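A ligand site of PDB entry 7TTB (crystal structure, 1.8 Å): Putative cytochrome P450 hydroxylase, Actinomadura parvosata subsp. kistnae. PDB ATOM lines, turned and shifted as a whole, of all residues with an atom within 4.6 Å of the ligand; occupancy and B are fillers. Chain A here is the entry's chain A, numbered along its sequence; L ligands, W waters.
The side-chain sulfur (SG) of Cys 332 binds an iron atom (FE1) of the ligand, at 2.4 Å.
O3 of the ligand lies within hydrogen-bond range of ND1 of His 330, at 2.6 Å.
NE2 of His 88 lies within hydrogen-bond range of O4 of the ligand (2.6 Å).
An oxygen (O2) of the ligand lies within salt-bridge range of the guanidinium group of Arg 277 (2.8 Å).
The guanidinium group of Arg 92 is in salt-bridge range of an oxygen (O4) of the ligand (2.8 Å).
An oxygen (O3) of the ligand is in hydrogen-bond range of the backbone NH (N) of Leu 81 (3.4 Å).
SG of Cys 332 lies close to N of Gly 334 (3.3 Å).
O of Phe 325 is in hydrogen-bond range of N of Cys 332 (2.9 Å).
NE2 of His 88 lies close to O of Ile 329 (3.4 Å).
NH1 of Arg 277 is in hydrogen-bond range of O of Asp 275 (3.1 Å).
The guanidinium group (NH1) of Arg 92 is in hydrogen-bond range of the backbone carbonyl oxygen (O) of Ile 329 (3.3 Å).
NZ of Lys 62 sits at hydrogen-bond distance from O of Leu 81.
O of Ser 224 lies within hydrogen-bond range of OG1 of Thr 229 (3.1 Å).
The backbone carbonyl oxygen (O) of Val 221 lies within hydrogen-bond range of the side-chain hydroxyl (OG) of Ser 225, 3.0 Å away.
C of Leu 80 touches O3 of the ligand (3.4 Å).
Tyr 99 touches the ligand.
Val 220 touches the ligand (CG1 to C31, 3.8 Å).
CG2 of Val 221 touches C26 of the ligand, at 3.6 Å.
CB of Ser 224 touches N3 of the ligand, at 3.5 Å.
CB of Gln 228 touches C15 of the ligand (3.6 Å).
Thr 229 touches the ligand.
Cys 232 touches the ligand (SG to C19, 3.2 Å).
Phe 271 touches the ligand.
Leu 274 touches the ligand.
CD1 of Leu 300 touches C9 of the ligand (3.5 Å).
Ala 324 touches the ligand (O to C9, 3.5 Å).
Phe 325 touches the ligand (C to C9, 3.5 Å).
Gly 326 touches the ligand.
Ile 329 touches the ligand.
Leu 333 touches the ligand.
CA of Gly 334 touches C22 of the ligand (3.5 Å).
Ala 338 touches the ligand.
Hydrophobic or aromatic side chains that line the ligand: Leu 80, Leu 81, His 88, Tyr 99, Val 220, Val 221, Phe 271, Leu 274, Leu 300, Phe 325, His 330, Leu 333 and Ala 338.
Of the 32 residues printed, 24 come within 4 Å of the ligand.
The nearest printed residue that does not touch the ligand is Val 270 (4.1 Å).
Water W2 bridges an oxygen (O1) of the ligand and the backbone NH of Asp 275.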
ATOM      1  N   LYS A  62     -13.552 -12.014  11.407  1.00  0.00           N
ATOM      2  CA  LYS A  62     -13.229 -11.599  12.763  1.00  0.00           C
ATOM      3  C   LYS A  62     -13.274 -12.794  13.698  1.00  0.00           C
ATOM      4  O   LYS A  62     -13.829 -12.726  14.796  1.00  0.00           O
ATOM      5  CB  LYS A  62     -14.178 -10.489  13.235  1.00  0.00           C
ATOM      6  CG  LYS A  62     -13.892  -9.157  12.554  1.00  0.00           C
ATOM      7  CD  LYS A  62     -14.629  -7.975  13.145  1.00  0.00           C
ATOM      8  CE  LYS A  62     -13.917  -7.418  14.353  1.00  0.00           C
ATOM      9  NZ  LYS A  62     -14.112  -8.252  15.564  1.00  0.00           N
ATOM     10  N   LEU A  80     -22.375  -6.232  16.674  1.00  0.00           N
ATOM     11  CA  LEU A  80     -22.033  -6.283  15.255  1.00  0.00           C
ATOM     12  C   LEU A  80     -20.560  -6.580  15.036  1.00  0.00           C
ATOM     13  O   LEU A  80     -20.196  -7.198  14.021  1.00  0.00           O
ATOM     14  CB  LEU A  80     -22.399  -4.958  14.575  1.00  0.00           C
ATOM     15  CG  LEU A  80     -23.859  -4.700  14.230  1.00  0.00           C
ATOM     16  CD1 LEU A  80     -24.098  -3.206  13.971  1.00  0.00           C
ATOM     17  CD2 LEU A  80     -24.271  -5.502  13.004  1.00  0.00           C
ATOM     18  N   LEU A  81     -19.694  -6.154  15.952  1.00  0.00           N
ATOM     19  CA  LEU A  81     -18.271  -6.358  15.767  1.00  0.00           C
ATOM     20  C   LEU A  81     -17.875  -7.827  15.813  1.00  0.00           C
ATOM     21  O   LEU A  81     -16.777  -8.164  15.387  1.00  0.00           O
ATOM     22  CB  LEU A  81     -17.469  -5.594  16.815  1.00  0.00           C
ATOM     23  CG  LEU A  81     -16.931  -4.231  16.392  1.00  0.00           C
ATOM     24  CD1 LEU A  81     -16.100  -3.644  17.523  1.00  0.00           C
ATOM     25  CD2 LEU A  81     -16.107  -4.313  15.110  1.00  0.00           C
ATOM     26  N   HIS A  88     -23.786 -10.392   9.816  1.00  0.00           N
ATOM     27  CA  HIS A  88     -23.456  -8.997  10.081  1.00  0.00           C
ATOM     28  C   HIS A  88     -24.336  -8.063   9.251  1.00  0.00           C
ATOM     29  O   HIS A  88     -24.927  -7.118   9.775  1.00  0.00           O
ATOM     30  CB  HIS A  88     -21.981  -8.738   9.784  1.00  0.00           C
ATOM     31  CG  HIS A  88     -21.598  -7.288   9.849  1.00  0.00           C
ATOM     32  ND1 HIS A  88     -21.606  -6.463   8.740  1.00  0.00           N
ATOM     33  CD2 HIS A  88     -21.238  -6.502  10.890  1.00  0.00           C
ATOM     34  CE1 HIS A  88     -21.241  -5.248   9.100  1.00  0.00           C
ATOM     35  NE2 HIS A  88     -21.013  -5.247  10.401  1.00  0.00           N
ATOM     36  N   ARG A  92     -26.921  -5.237  10.687  1.00  0.00           N
ATOM     37  CA  ARG A  92     -26.554  -3.855  10.415  1.00  0.00           C
ATOM     38  C   ARG A  92     -27.626  -3.144   9.604  1.00  0.00           C
ATOM     39  O   ARG A  92     -27.952  -1.989   9.876  1.00  0.00           O
ATOM     40  CB  ARG A  92     -25.210  -3.788   9.700  1.00  0.00           C
ATOM     41  CG  ARG A  92     -24.793  -2.373   9.349  1.00  0.00           C
ATOM     42  CD  ARG A  92     -23.383  -2.054   9.793  1.00  0.00           C
ATOM     43  NE  ARG A  92     -23.061  -0.653   9.504  1.00  0.00           N
ATOM     44  CZ  ARG A  92     -21.959  -0.028   9.904  1.00  0.00           C
ATOM     45  NH1 ARG A  92     -21.054  -0.657  10.632  1.00  0.00           N
ATOM     46  NH2 ARG A  92     -21.777   1.250   9.587  1.00  0.00           N
ATOM     47  N   TYR A  99     -29.244   6.271  11.763  1.00  0.00           N
ATOM     48  CA  TYR A  99     -28.171   7.252  11.631  1.00  0.00           C
ATOM     49  C   TYR A  99     -28.241   8.016  10.307  1.00  0.00           C
ATOM     50  O   TYR A  99     -27.272   8.675   9.931  1.00  0.00           O
ATOM     51  CB  TYR A  99     -26.814   6.570  11.772  1.00  0.00           C
ATOM     52  CG  TYR A  99     -26.690   5.718  13.022  1.00  0.00           C
ATOM     53  CD1 TYR A  99     -27.248   4.446  13.079  1.00  0.00           C
ATOM     54  CD2 TYR A  99     -26.035   6.195  14.159  1.00  0.00           C
ATOM     55  CE1 TYR A  99     -27.156   3.662  14.208  1.00  0.00           C
ATOM     56  CE2 TYR A  99     -25.937   5.408  15.300  1.00  0.00           C
ATOM     57  CZ  TYR A  99     -26.503   4.147  15.316  1.00  0.00           C
ATOM     58  OH  TYR A  99     -26.411   3.362  16.445  1.00  0.00           O
ATOM     59  N   VAL A 220     -23.925  -1.818  23.590  1.00  0.00           N
ATOM     60  CA  VAL A 220     -22.833  -1.322  22.756  1.00  0.00           C
ATOM     61  C   VAL A 220     -22.904   0.199  22.641  1.00  0.00           C
ATOM     62  O   VAL A 220     -21.871   0.885  22.667  1.00  0.00           O
ATOM     63  CB  VAL A 220     -22.853  -1.995  21.378  1.00  0.00           C
ATOM     64  CG1 VAL A 220     -21.861  -1.330  20.442  1.00  0.00           C
ATOM     65  CG2 VAL A 220     -22.532  -3.481  21.508  1.00  0.00           C
ATOM     66  N   VAL A 221     -24.107   0.740  22.441  1.00  0.00           N
ATOM     67  CA  VAL A 221     -24.269   2.181  22.286  1.00  0.00           C
ATOM     68  C   VAL A 221     -23.844   2.889  23.558  1.00  0.00           C
ATOM     69  O   VAL A 221     -23.054   3.836  23.533  1.00  0.00           O
ATOM     70  CB  VAL A 221     -25.719   2.530  21.893  1.00  0.00           C
ATOM     71  CG1 VAL A 221     -25.933   4.042  21.894  1.00  0.00           C
ATOM     72  CG2 VAL A 221     -26.049   1.944  20.528  1.00  0.00           C
ATOM     73  N   SER A 224     -20.069   2.556  23.835  1.00  0.00           N
ATOM     74  CA  SER A 224     -19.361   3.428  22.902  1.00  0.00           C
ATOM     75  C   SER A 224     -19.505   4.898  23.265  1.00  0.00           C
ATOM     76  O   SER A 224     -18.640   5.698  22.901  1.00  0.00           O
ATOM     77  CB  SER A 224     -19.862   3.181  21.472  1.00  0.00           C
ATOM     78  OG  SER A 224     -19.361   1.960  20.959  1.00  0.00           O
ATOM     79  N   SER A 225     -20.569   5.261  23.980  1.00  0.00           N
ATOM     80  CA  SER A 225     -20.758   6.634  24.412  1.00  0.00           C
ATOM     81  C   SER A 225     -19.924   6.948  25.657  1.00  0.00           C
ATOM     82  O   SER A 225     -19.239   7.971  25.710  1.00  0.00           O
ATOM     83  CB  SER A 225     -22.237   6.906  24.684  1.00  0.00           C
ATOM     84  OG  SER A 225     -22.998   6.816  23.488  1.00  0.00           O
ATOM     85  N   GLN A 228     -15.646   5.626  24.243  1.00  0.00           N
ATOM     86  CA  GLN A 228     -15.040   6.359  23.130  1.00  0.00           C
ATOM     87  C   GLN A 228     -15.424   7.833  23.149  1.00  0.00           C
ATOM     88  O   GLN A 228     -14.564   8.711  23.048  1.00  0.00           O
ATOM     89  CB  GLN A 228     -15.441   5.719  21.799  1.00  0.00           C
ATOM     90  CG  GLN A 228     -14.663   4.469  21.411  1.00  0.00           C
ATOM     91  CD  GLN A 228     -15.199   3.214  22.076  1.00  0.00           C
ATOM     92  OE1 GLN A 228     -16.054   3.274  22.958  1.00  0.00           O
ATOM     93  NE2 GLN A 228     -14.700   2.059  21.642  1.00  0.00           N
ATOM     94  N   THR A 229     -16.729   8.123  23.247  1.00  0.00           N
ATOM     95  CA  THR A 229     -17.194   9.488  23.050  1.00  0.00           C
ATOM     96  C   THR A 229     -16.773  10.375  24.221  1.00  0.00           C
ATOM     97  O   THR A 229     -16.284  11.488  24.025  1.00  0.00           O
ATOM     98  CB  THR A 229     -18.719   9.504  22.871  1.00  0.00           C
ATOM     99  OG1 THR A 229     -19.072   8.565  21.841  1.00  0.00           O
ATOM    100  CG2 THR A 229     -19.194  10.881  22.477  1.00  0.00           C
ATOM    101  N   CYS A 232     -13.135  11.220  23.835  1.00  0.00           N
ATOM    102  CA  CYS A 232     -12.957  12.282  22.853  1.00  0.00           C
ATOM    103  C   CYS A 232     -13.327  13.635  23.438  1.00  0.00           C
ATOM    104  O   CYS A 232     -12.618  14.628  23.231  1.00  0.00           O
ATOM    105  CB  CYS A 232     -13.801  11.998  21.603  1.00  0.00           C
ATOM    106  SG  CYS A 232     -13.123  10.746  20.527  1.00  0.00           S
ATOM    107  N   VAL A 265     -10.483  13.721  16.332  1.00  0.00           N
ATOM    108  CA  VAL A 265     -10.538  12.263  16.428  1.00  0.00           C
ATOM    109  C   VAL A 265      -9.299  11.628  15.782  1.00  0.00           C
ATOM    110  O   VAL A 265      -8.818  10.583  16.253  1.00  0.00           O
ATOM    111  CB  VAL A 265     -11.845  11.678  15.836  1.00  0.00           C
ATOM    112  CG1 VAL A 265     -13.040  12.230  16.563  1.00  0.00           C
ATOM    113  CG2 VAL A 265     -11.952  11.936  14.326  1.00  0.00           C
ATOM    114  N   VAL A 270      -8.629   7.610  19.976  1.00  0.00           N
ATOM    115  CA  VAL A 270      -8.971   6.970  21.246  1.00  0.00           C
ATOM    116  C   VAL A 270      -9.217   5.495  21.053  1.00  0.00           C
ATOM    117  O   VAL A 270      -8.971   4.688  21.952  1.00  0.00           O
ATOM    118  CB  VAL A 270     -10.182   7.660  21.923  1.00  0.00           C
ATOM    119  CG1 VAL A 270      -9.923   9.149  22.105  1.00  0.00           C
ATOM    120  CG2 VAL A 270     -11.483   7.416  21.149  1.00  0.00           C
ATOM    121  N   PHE A 271      -9.712   5.104  19.880  1.00  0.00           N
ATOM    122  CA  PHE A 271      -9.824   3.700  19.510  1.00  0.00           C
ATOM    123  C   PHE A 271      -8.525   3.400  18.760  1.00  0.00           C
ATOM    124  O   PHE A 271      -8.382   3.718  17.586  1.00  0.00           O
ATOM    125  CB  PHE A 271     -11.067   3.486  18.647  1.00  0.00           C
ATOM    126  CG  PHE A 271     -11.573   2.078  18.613  1.00  0.00           C
ATOM    127  CD1 PHE A 271     -10.721   0.984  18.580  1.00  0.00           C
ATOM    128  CD2 PHE A 271     -12.932   1.848  18.560  1.00  0.00           C
ATOM    129  CE1 PHE A 271     -11.208  -0.306  18.516  1.00  0.00           C
ATOM    130  CE2 PHE A 271     -13.429   0.550  18.491  1.00  0.00           C
ATOM    131  CZ  PHE A 271     -12.568  -0.518  18.475  1.00  0.00           C
ATOM    132  N   LEU A 274      -7.453  -2.300  16.401  1.00  0.00           N
ATOM    133  CA  LEU A 274      -8.642  -3.068  16.096  1.00  0.00           C
ATOM    134  C   LEU A 274      -8.467  -4.539  16.411  1.00  0.00           C
ATOM    135  O   LEU A 274      -7.356  -5.079  16.424  1.00  0.00           O
ATOM    136  CB  LEU A 274      -9.019  -2.903  14.621  1.00  0.00           C
ATOM    137  CG  LEU A 274      -9.328  -1.485  14.171  1.00  0.00           C
ATOM    138  CD1 LEU A 274      -9.845  -1.507  12.733  1.00  0.00           C
ATOM    139  CD2 LEU A 274     -10.338  -0.816  15.102  1.00  0.00           C
ATOM    140  N   ASP A 275      -9.601  -5.190  16.681  1.00  0.00           N
ATOM    141  CA  ASP A 275      -9.673  -6.644  16.731  1.00  0.00           C
ATOM    142  C   ASP A 275      -8.995  -7.230  15.483  1.00  0.00           C
ATOM    143  O   ASP A 275      -9.156  -6.686  14.388  1.00  0.00           O
ATOM    144  CB  ASP A 275     -11.131  -7.124  16.745  1.00  0.00           C
ATOM    145  CG  ASP A 275     -11.892  -6.691  17.973  1.00  0.00           C
ATOM    146  OD1 ASP A 275     -11.277  -6.495  19.044  1.00  0.00           O
ATOM    147  OD2 ASP A 275     -13.137  -6.578  17.849  1.00  0.00           O
ATOM    148  N   ARG A 277      -8.024  -9.220  12.116  1.00  0.00           N
ATOM    149  CA  ARG A 277      -8.659  -9.734  10.915  1.00  0.00           C
ATOM    150  C   ARG A 277      -7.843 -10.927  10.436  1.00  0.00           C
ATOM    151  O   ARG A 277      -6.646 -10.781  10.165  1.00  0.00           O
ATOM    152  CB  ARG A 277      -8.737  -8.663   9.818  1.00  0.00           C
ATOM    153  CG  ARG A 277     -10.064  -7.934   9.736  1.00  0.00           C
ATOM    154  CD  ARG A 277     -10.364  -7.114  10.971  1.00  0.00           C
ATOM    155  NE  ARG A 277     -11.525  -6.265  10.748  1.00  0.00           N
ATOM    156  CZ  ARG A 277     -11.996  -5.388  11.629  1.00  0.00           C
ATOM    157  NH1 ARG A 277     -11.415  -5.238  12.807  1.00  0.00           N
ATOM    158  NH2 ARG A 277     -13.062  -4.661  11.323  1.00  0.00           N
ATOM    159  N   LEU A 300      -4.942   1.955  14.243  1.00  0.00           N
ATOM    160  CA  LEU A 300      -5.464   3.252  13.837  1.00  0.00           C
ATOM    161  C   LEU A 300      -4.570   4.367  14.346  1.00  0.00           C
ATOM    162  O   LEU A 300      -4.334   5.364  13.647  1.00  0.00           O
ATOM    163  CB  LEU A 300      -6.896   3.440  14.345  1.00  0.00           C
ATOM    164  CG  LEU A 300      -7.861   2.297  14.011  1.00  0.00           C
ATOM    165  CD1 LEU A 300      -9.293   2.684  14.381  1.00  0.00           C
ATOM    166  CD2 LEU A 300      -7.799   1.919  12.526  1.00  0.00           C
ATOM    167  N   ALA A 324      -9.924   6.988  12.048  1.00  0.00           N
ATOM    168  CA  ALA A 324     -10.321   6.975  13.446  1.00  0.00           C
ATOM    169  C   ALA A 324     -11.628   6.227  13.676  1.00  0.00           C
ATOM    170  O   ALA A 324     -11.877   5.730  14.779  1.00  0.00           O
ATOM    171  CB  ALA A 324     -10.433   8.406  13.983  1.00  0.00           C
ATOM    172  N   PHE A 325     -12.496   6.155  12.655  1.00  0.00           N
ATOM    173  CA  PHE A 325     -13.761   5.427  12.745  1.00  0.00           C
ATOM    174  C   PHE A 325     -13.723   4.109  11.982  1.00  0.00           C
ATOM    175  O   PHE A 325     -14.770   3.499  11.742  1.00  0.00           O
ATOM    176  CB  PHE A 325     -14.930   6.277  12.235  1.00  0.00           C
ATOM    177  CG  PHE A 325     -15.294   7.436  13.122  1.00  0.00           C
ATOM    178  CD1 PHE A 325     -15.858   7.228  14.362  1.00  0.00           C
ATOM    179  CD2 PHE A 325     -15.084   8.743  12.697  1.00  0.00           C
ATOM    180  CE1 PHE A 325     -16.210   8.290  15.176  1.00  0.00           C
ATOM    181  CE2 PHE A 325     -15.428   9.803  13.500  1.00  0.00           C
ATOM    182  CZ  PHE A 325     -15.991   9.595  14.739  1.00  0.00           C
ATOM    183  N   GLY A 326     -12.544   3.643  11.611  1.00  0.00           N
ATOM    184  CA  GLY A 326     -12.454   2.416  10.853  1.00  0.00           C
ATOM    185  C   GLY A 326     -12.797   2.629   9.389  1.00  0.00           C
ATOM    186  O   GLY A 326     -12.729   3.750   8.845  1.00  0.00           O
ATOM    187  N   ILE A 329     -17.004  -2.744   6.103  1.00  0.00           N
ATOM    188  CA  ILE A 329     -18.338  -3.116   6.567  1.00  0.00           C
ATOM    189  C   ILE A 329     -18.511  -2.880   8.053  1.00  0.00           C
ATOM    190  O   ILE A 329     -19.647  -2.709   8.508  1.00  0.00           O
ATOM    191  CB  ILE A 329     -18.662  -4.585   6.228  1.00  0.00           C
ATOM    192  CG1 ILE A 329     -17.729  -5.537   6.977  1.00  0.00           C
ATOM    193  CG2 ILE A 329     -18.590  -4.811   4.717  1.00  0.00           C
ATOM    194  CD1 ILE A 329     -18.137  -7.024   6.844  1.00  0.00           C
ATOM    195  N   HIS A 330     -17.431  -2.859   8.829  1.00  0.00           N
ATOM    196  CA  HIS A 330     -17.501  -2.624  10.262  1.00  0.00           C
ATOM    197  C   HIS A 330     -17.252  -1.164  10.632  1.00  0.00           C
ATOM    198  O   HIS A 330     -17.161  -0.842  11.825  1.00  0.00           O
ATOM    199  CB  HIS A 330     -16.517  -3.528  11.007  1.00  0.00           C
ATOM    200  CG  HIS A 330     -16.906  -4.978  11.015  1.00  0.00           C
ATOM    201  ND1 HIS A 330     -17.894  -5.485  11.826  1.00  0.00           N
ATOM    202  CD2 HIS A 330     -16.415  -6.033  10.315  1.00  0.00           C
ATOM    203  CE1 HIS A 330     -18.006  -6.783  11.628  1.00  0.00           C
ATOM    204  NE2 HIS A 330     -17.118  -7.148  10.706  1.00  0.00           N
ATOM    205  N   HIS A 331     -17.164  -0.270   9.629  1.00  0.00           N
ATOM    206  CA  HIS A 331     -16.985   1.162   9.874  1.00  0.00           C
ATOM    207  C   HIS A 331     -17.981   1.659  10.911  1.00  0.00           C
ATOM    208  O   HIS A 331     -19.173   1.349  10.854  1.00  0.00           O
ATOM    209  CB  HIS A 331     -17.191   1.912   8.560  1.00  0.00           C
ATOM    210  CG  HIS A 331     -17.211   3.403   8.707  1.00  0.00           C
ATOM    211  ND1 HIS A 331     -18.382   4.127   8.744  1.00  0.00           N
ATOM    212  CD2 HIS A 331     -16.203   4.307   8.814  1.00  0.00           C
ATOM    213  CE1 HIS A 331     -18.091   5.418   8.879  1.00  0.00           C
ATOM    214  NE2 HIS A 331     -16.782   5.544   8.923  1.00  0.00           N
ATOM    215  N   CYS A 332     -17.484   2.481  11.845  1.00  0.00           N
ATOM    216  CA  CYS A 332     -18.261   2.866  13.022  1.00  0.00           C
ATOM    217  C   CYS A 332     -19.699   3.196  12.675  1.00  0.00           C
ATOM    218  O   CYS A 332     -19.979   4.164  11.967  1.00  0.00           O
ATOM    219  CB  CYS A 332     -17.616   4.062  13.704  1.00  0.00           C
ATOM    220  SG  CYS A 332     -18.620   4.629  15.106  1.00  0.00           S
ATOM    221  N   LEU A 333     -20.623   2.395  13.206  1.00  0.00           N
ATOM    222  CA  LEU A 333     -22.043   2.639  12.958  1.00  0.00           C
ATOM    223  C   LEU A 333     -22.494   3.967  13.573  1.00  0.00           C
ATOM    224  O   LEU A 333     -23.406   4.615  13.049  1.00  0.00           O
ATOM    225  CB  LEU A 333     -22.859   1.488  13.524  1.00  0.00           C
ATOM    226  CG  LEU A 333     -24.378   1.514  13.336  1.00  0.00           C
ATOM    227  CD1 LEU A 333     -24.720   1.391  11.870  1.00  0.00           C
ATOM    228  CD2 LEU A 333     -25.045   0.419  14.139  1.00  0.00           C
ATOM    229  N   GLY A 334     -21.860   4.380  14.659  1.00  0.00           N
ATOM    230  CA  GLY A 334     -22.251   5.601  15.320  1.00  0.00           C
ATOM    231  C   GLY A 334     -21.560   6.860  14.863  1.00  0.00           C
ATOM    232  O   GLY A 334     -21.796   7.922  15.453  1.00  0.00           O
ATOM    233  N   LEU A 337     -23.564  10.113  14.690  1.00  0.00           N
ATOM    234  CA  LEU A 337     -23.911  10.643  16.009  1.00  0.00           C
ATOM    235  C   LEU A 337     -22.679  11.230  16.698  1.00  0.00           C
ATOM    236  O   LEU A 337     -22.732  12.338  17.250  1.00  0.00           O
ATOM    237  CB  LEU A 337     -24.529   9.545  16.854  1.00  0.00           C
ATOM    238  CG  LEU A 337     -24.902   9.938  18.288  1.00  0.00           C
ATOM    239  CD1 LEU A 337     -25.872  11.093  18.292  1.00  0.00           C
ATOM    240  CD2 LEU A 337     -25.499   8.755  19.027  1.00  0.00           C
ATOM    241  N   ALA A 338     -21.583  10.483  16.712  1.00  0.00           N
ATOM    242  CA  ALA A 338     -20.359  10.950  17.370  1.00  0.00           C
ATOM    243  C   ALA A 338     -19.886  12.265  16.762  1.00  0.00           C
ATOM    244  O   ALA A 338     -19.512  13.195  17.482  1.00  0.00           O
ATOM    245  CB  ALA A 338     -19.264   9.892  17.247  1.00  0.00           C
ATOM    246  N   LEU A 342     -19.844  15.645  19.064  1.00  0.00           N
ATOM    247  CA  LEU A 342     -18.577  16.296  19.334  1.00  0.00           C
ATOM    248  C   LEU A 342     -18.541  17.711  18.765  1.00  0.00           C
ATOM    249  O   LEU A 342     -17.996  18.632  19.400  1.00  0.00           O
ATOM    250  CB  LEU A 342     -17.420  15.474  18.763  1.00  0.00           C
ATOM    251  CG  LEU A 342     -17.201  14.102  19.427  1.00  0.00           C
ATOM    252  CD1 LEU A 342     -16.113  13.339  18.686  1.00  0.00           C
ATOM    253  CD2 LEU A 342     -16.855  14.241  20.918  1.00  0.00           C
HETATM  254  C1  LIG L   1     -17.365   0.373  15.367  1.00  0.00           C
HETATM  255  C2  LIG L   1     -14.626   4.172  16.645  1.00  0.00           C
HETATM  256  C3  LIG L   1     -18.462   6.128  18.810  1.00  0.00           C
HETATM  257  C4  LIG L   1     -21.209   2.328  17.631  1.00  0.00           C
HETATM  258  C5  LIG L   1     -16.289   1.237  15.476  1.00  0.00           C
HETATM  259  C6  LIG L   1     -14.973   1.068  14.880  1.00  0.00           C
HETATM  260  C7  LIG L   1     -14.229   2.125  15.238  1.00  0.00           C
HETATM  261  C8  LIG L   1     -15.046   2.987  16.071  1.00  0.00           C
HETATM  262  C9  LIG L   1     -12.753   2.393  14.863  1.00  0.00           C
HETATM  263  C10 LIG L   1     -14.516  -0.109  13.988  1.00  0.00           C
HETATM  264  C11 LIG L   1     -13.993  -1.261  14.841  1.00  0.00           C
HETATM  265  C12 LIG L   1     -13.491  -2.381  13.965  1.00  0.00           C
HETATM  266  O1  LIG L   1     -12.867  -3.344  14.501  1.00  0.00           O
HETATM  267  O2  LIG L   1     -13.691  -2.339  12.717  1.00  0.00           O
HETATM  268  C13 LIG L   1     -15.421   5.044  17.336  1.00  0.00           C
HETATM  269  C14 LIG L   1     -15.032   6.349  17.863  1.00  0.00           C
HETATM  270  C15 LIG L   1     -16.108   6.870  18.468  1.00  0.00           C
HETATM  271  C16 LIG L   1     -17.196   5.930  18.325  1.00  0.00           C
HETATM  272  C17 LIG L   1     -13.608   6.947  17.707  1.00  0.00           C
HETATM  273  C18 LIG L   1     -16.296   8.225  19.187  1.00  0.00           C
HETATM  274  C19 LIG L   1     -15.465   9.261  19.014  1.00  0.00           C
HETATM  275  C20 LIG L   1     -19.544   5.325  18.616  1.00  0.00           C
HETATM  276  C21 LIG L   1     -20.914   5.683  18.921  1.00  0.00           C
HETATM  277  C22 LIG L   1     -21.697   4.653  18.602  1.00  0.00           C
HETATM  278  C23 LIG L   1     -20.845   3.577  18.078  1.00  0.00           C
HETATM  279  C24 LIG L   1     -21.365   7.043  19.504  1.00  0.00           C
HETATM  280  C25 LIG L   1     -23.239   4.656  18.781  1.00  0.00           C
HETATM  281  C26 LIG L   1     -24.026   3.768  18.179  1.00  0.00           C
HETATM  282  C27 LIG L   1     -20.378   1.454  16.946  1.00  0.00           C
HETATM  283  C28 LIG L   1     -20.747   0.132  16.486  1.00  0.00           C
HETATM  284  C29 LIG L   1     -19.694  -0.410  15.863  1.00  0.00           C
HETATM  285  C30 LIG L   1     -18.618   0.556  15.907  1.00  0.00           C
HETATM  286  C31 LIG L   1     -22.120  -0.514  16.711  1.00  0.00           C
HETATM  287  C32 LIG L   1     -19.618  -1.804  15.200  1.00  0.00           C
HETATM  288  C33 LIG L   1     -20.098  -1.698  13.758  1.00  0.00           C
HETATM  289  C34 LIG L   1     -19.926  -2.989  12.989  1.00  0.00           C
HETATM  290  O3  LIG L   1     -19.143  -3.875  13.448  1.00  0.00           O
HETATM  291  O4  LIG L   1     -20.563  -3.127  11.909  1.00  0.00           O
HETATM  292  N1  LIG L   1     -16.296   2.414  16.179  1.00  0.00           N
HETATM  293  N2  LIG L   1     -16.749   4.825  17.641  1.00  0.00           N
HETATM  294  N3  LIG L   1     -19.544   4.037  18.103  1.00  0.00           N
HETATM  295  N4  LIG L   1     -19.064   1.681  16.578  1.00  0.00           N
HETATM  296 FE1  LIG L   1     -17.957   3.343  17.002  1.00  0.00          FE
HETATM  297  O   HOH W   1     -13.770  -0.851  10.467  1.00  0.00           O
HETATM  298  O   HOH W   2     -12.022  -3.866  16.945  1.00  0.00           O
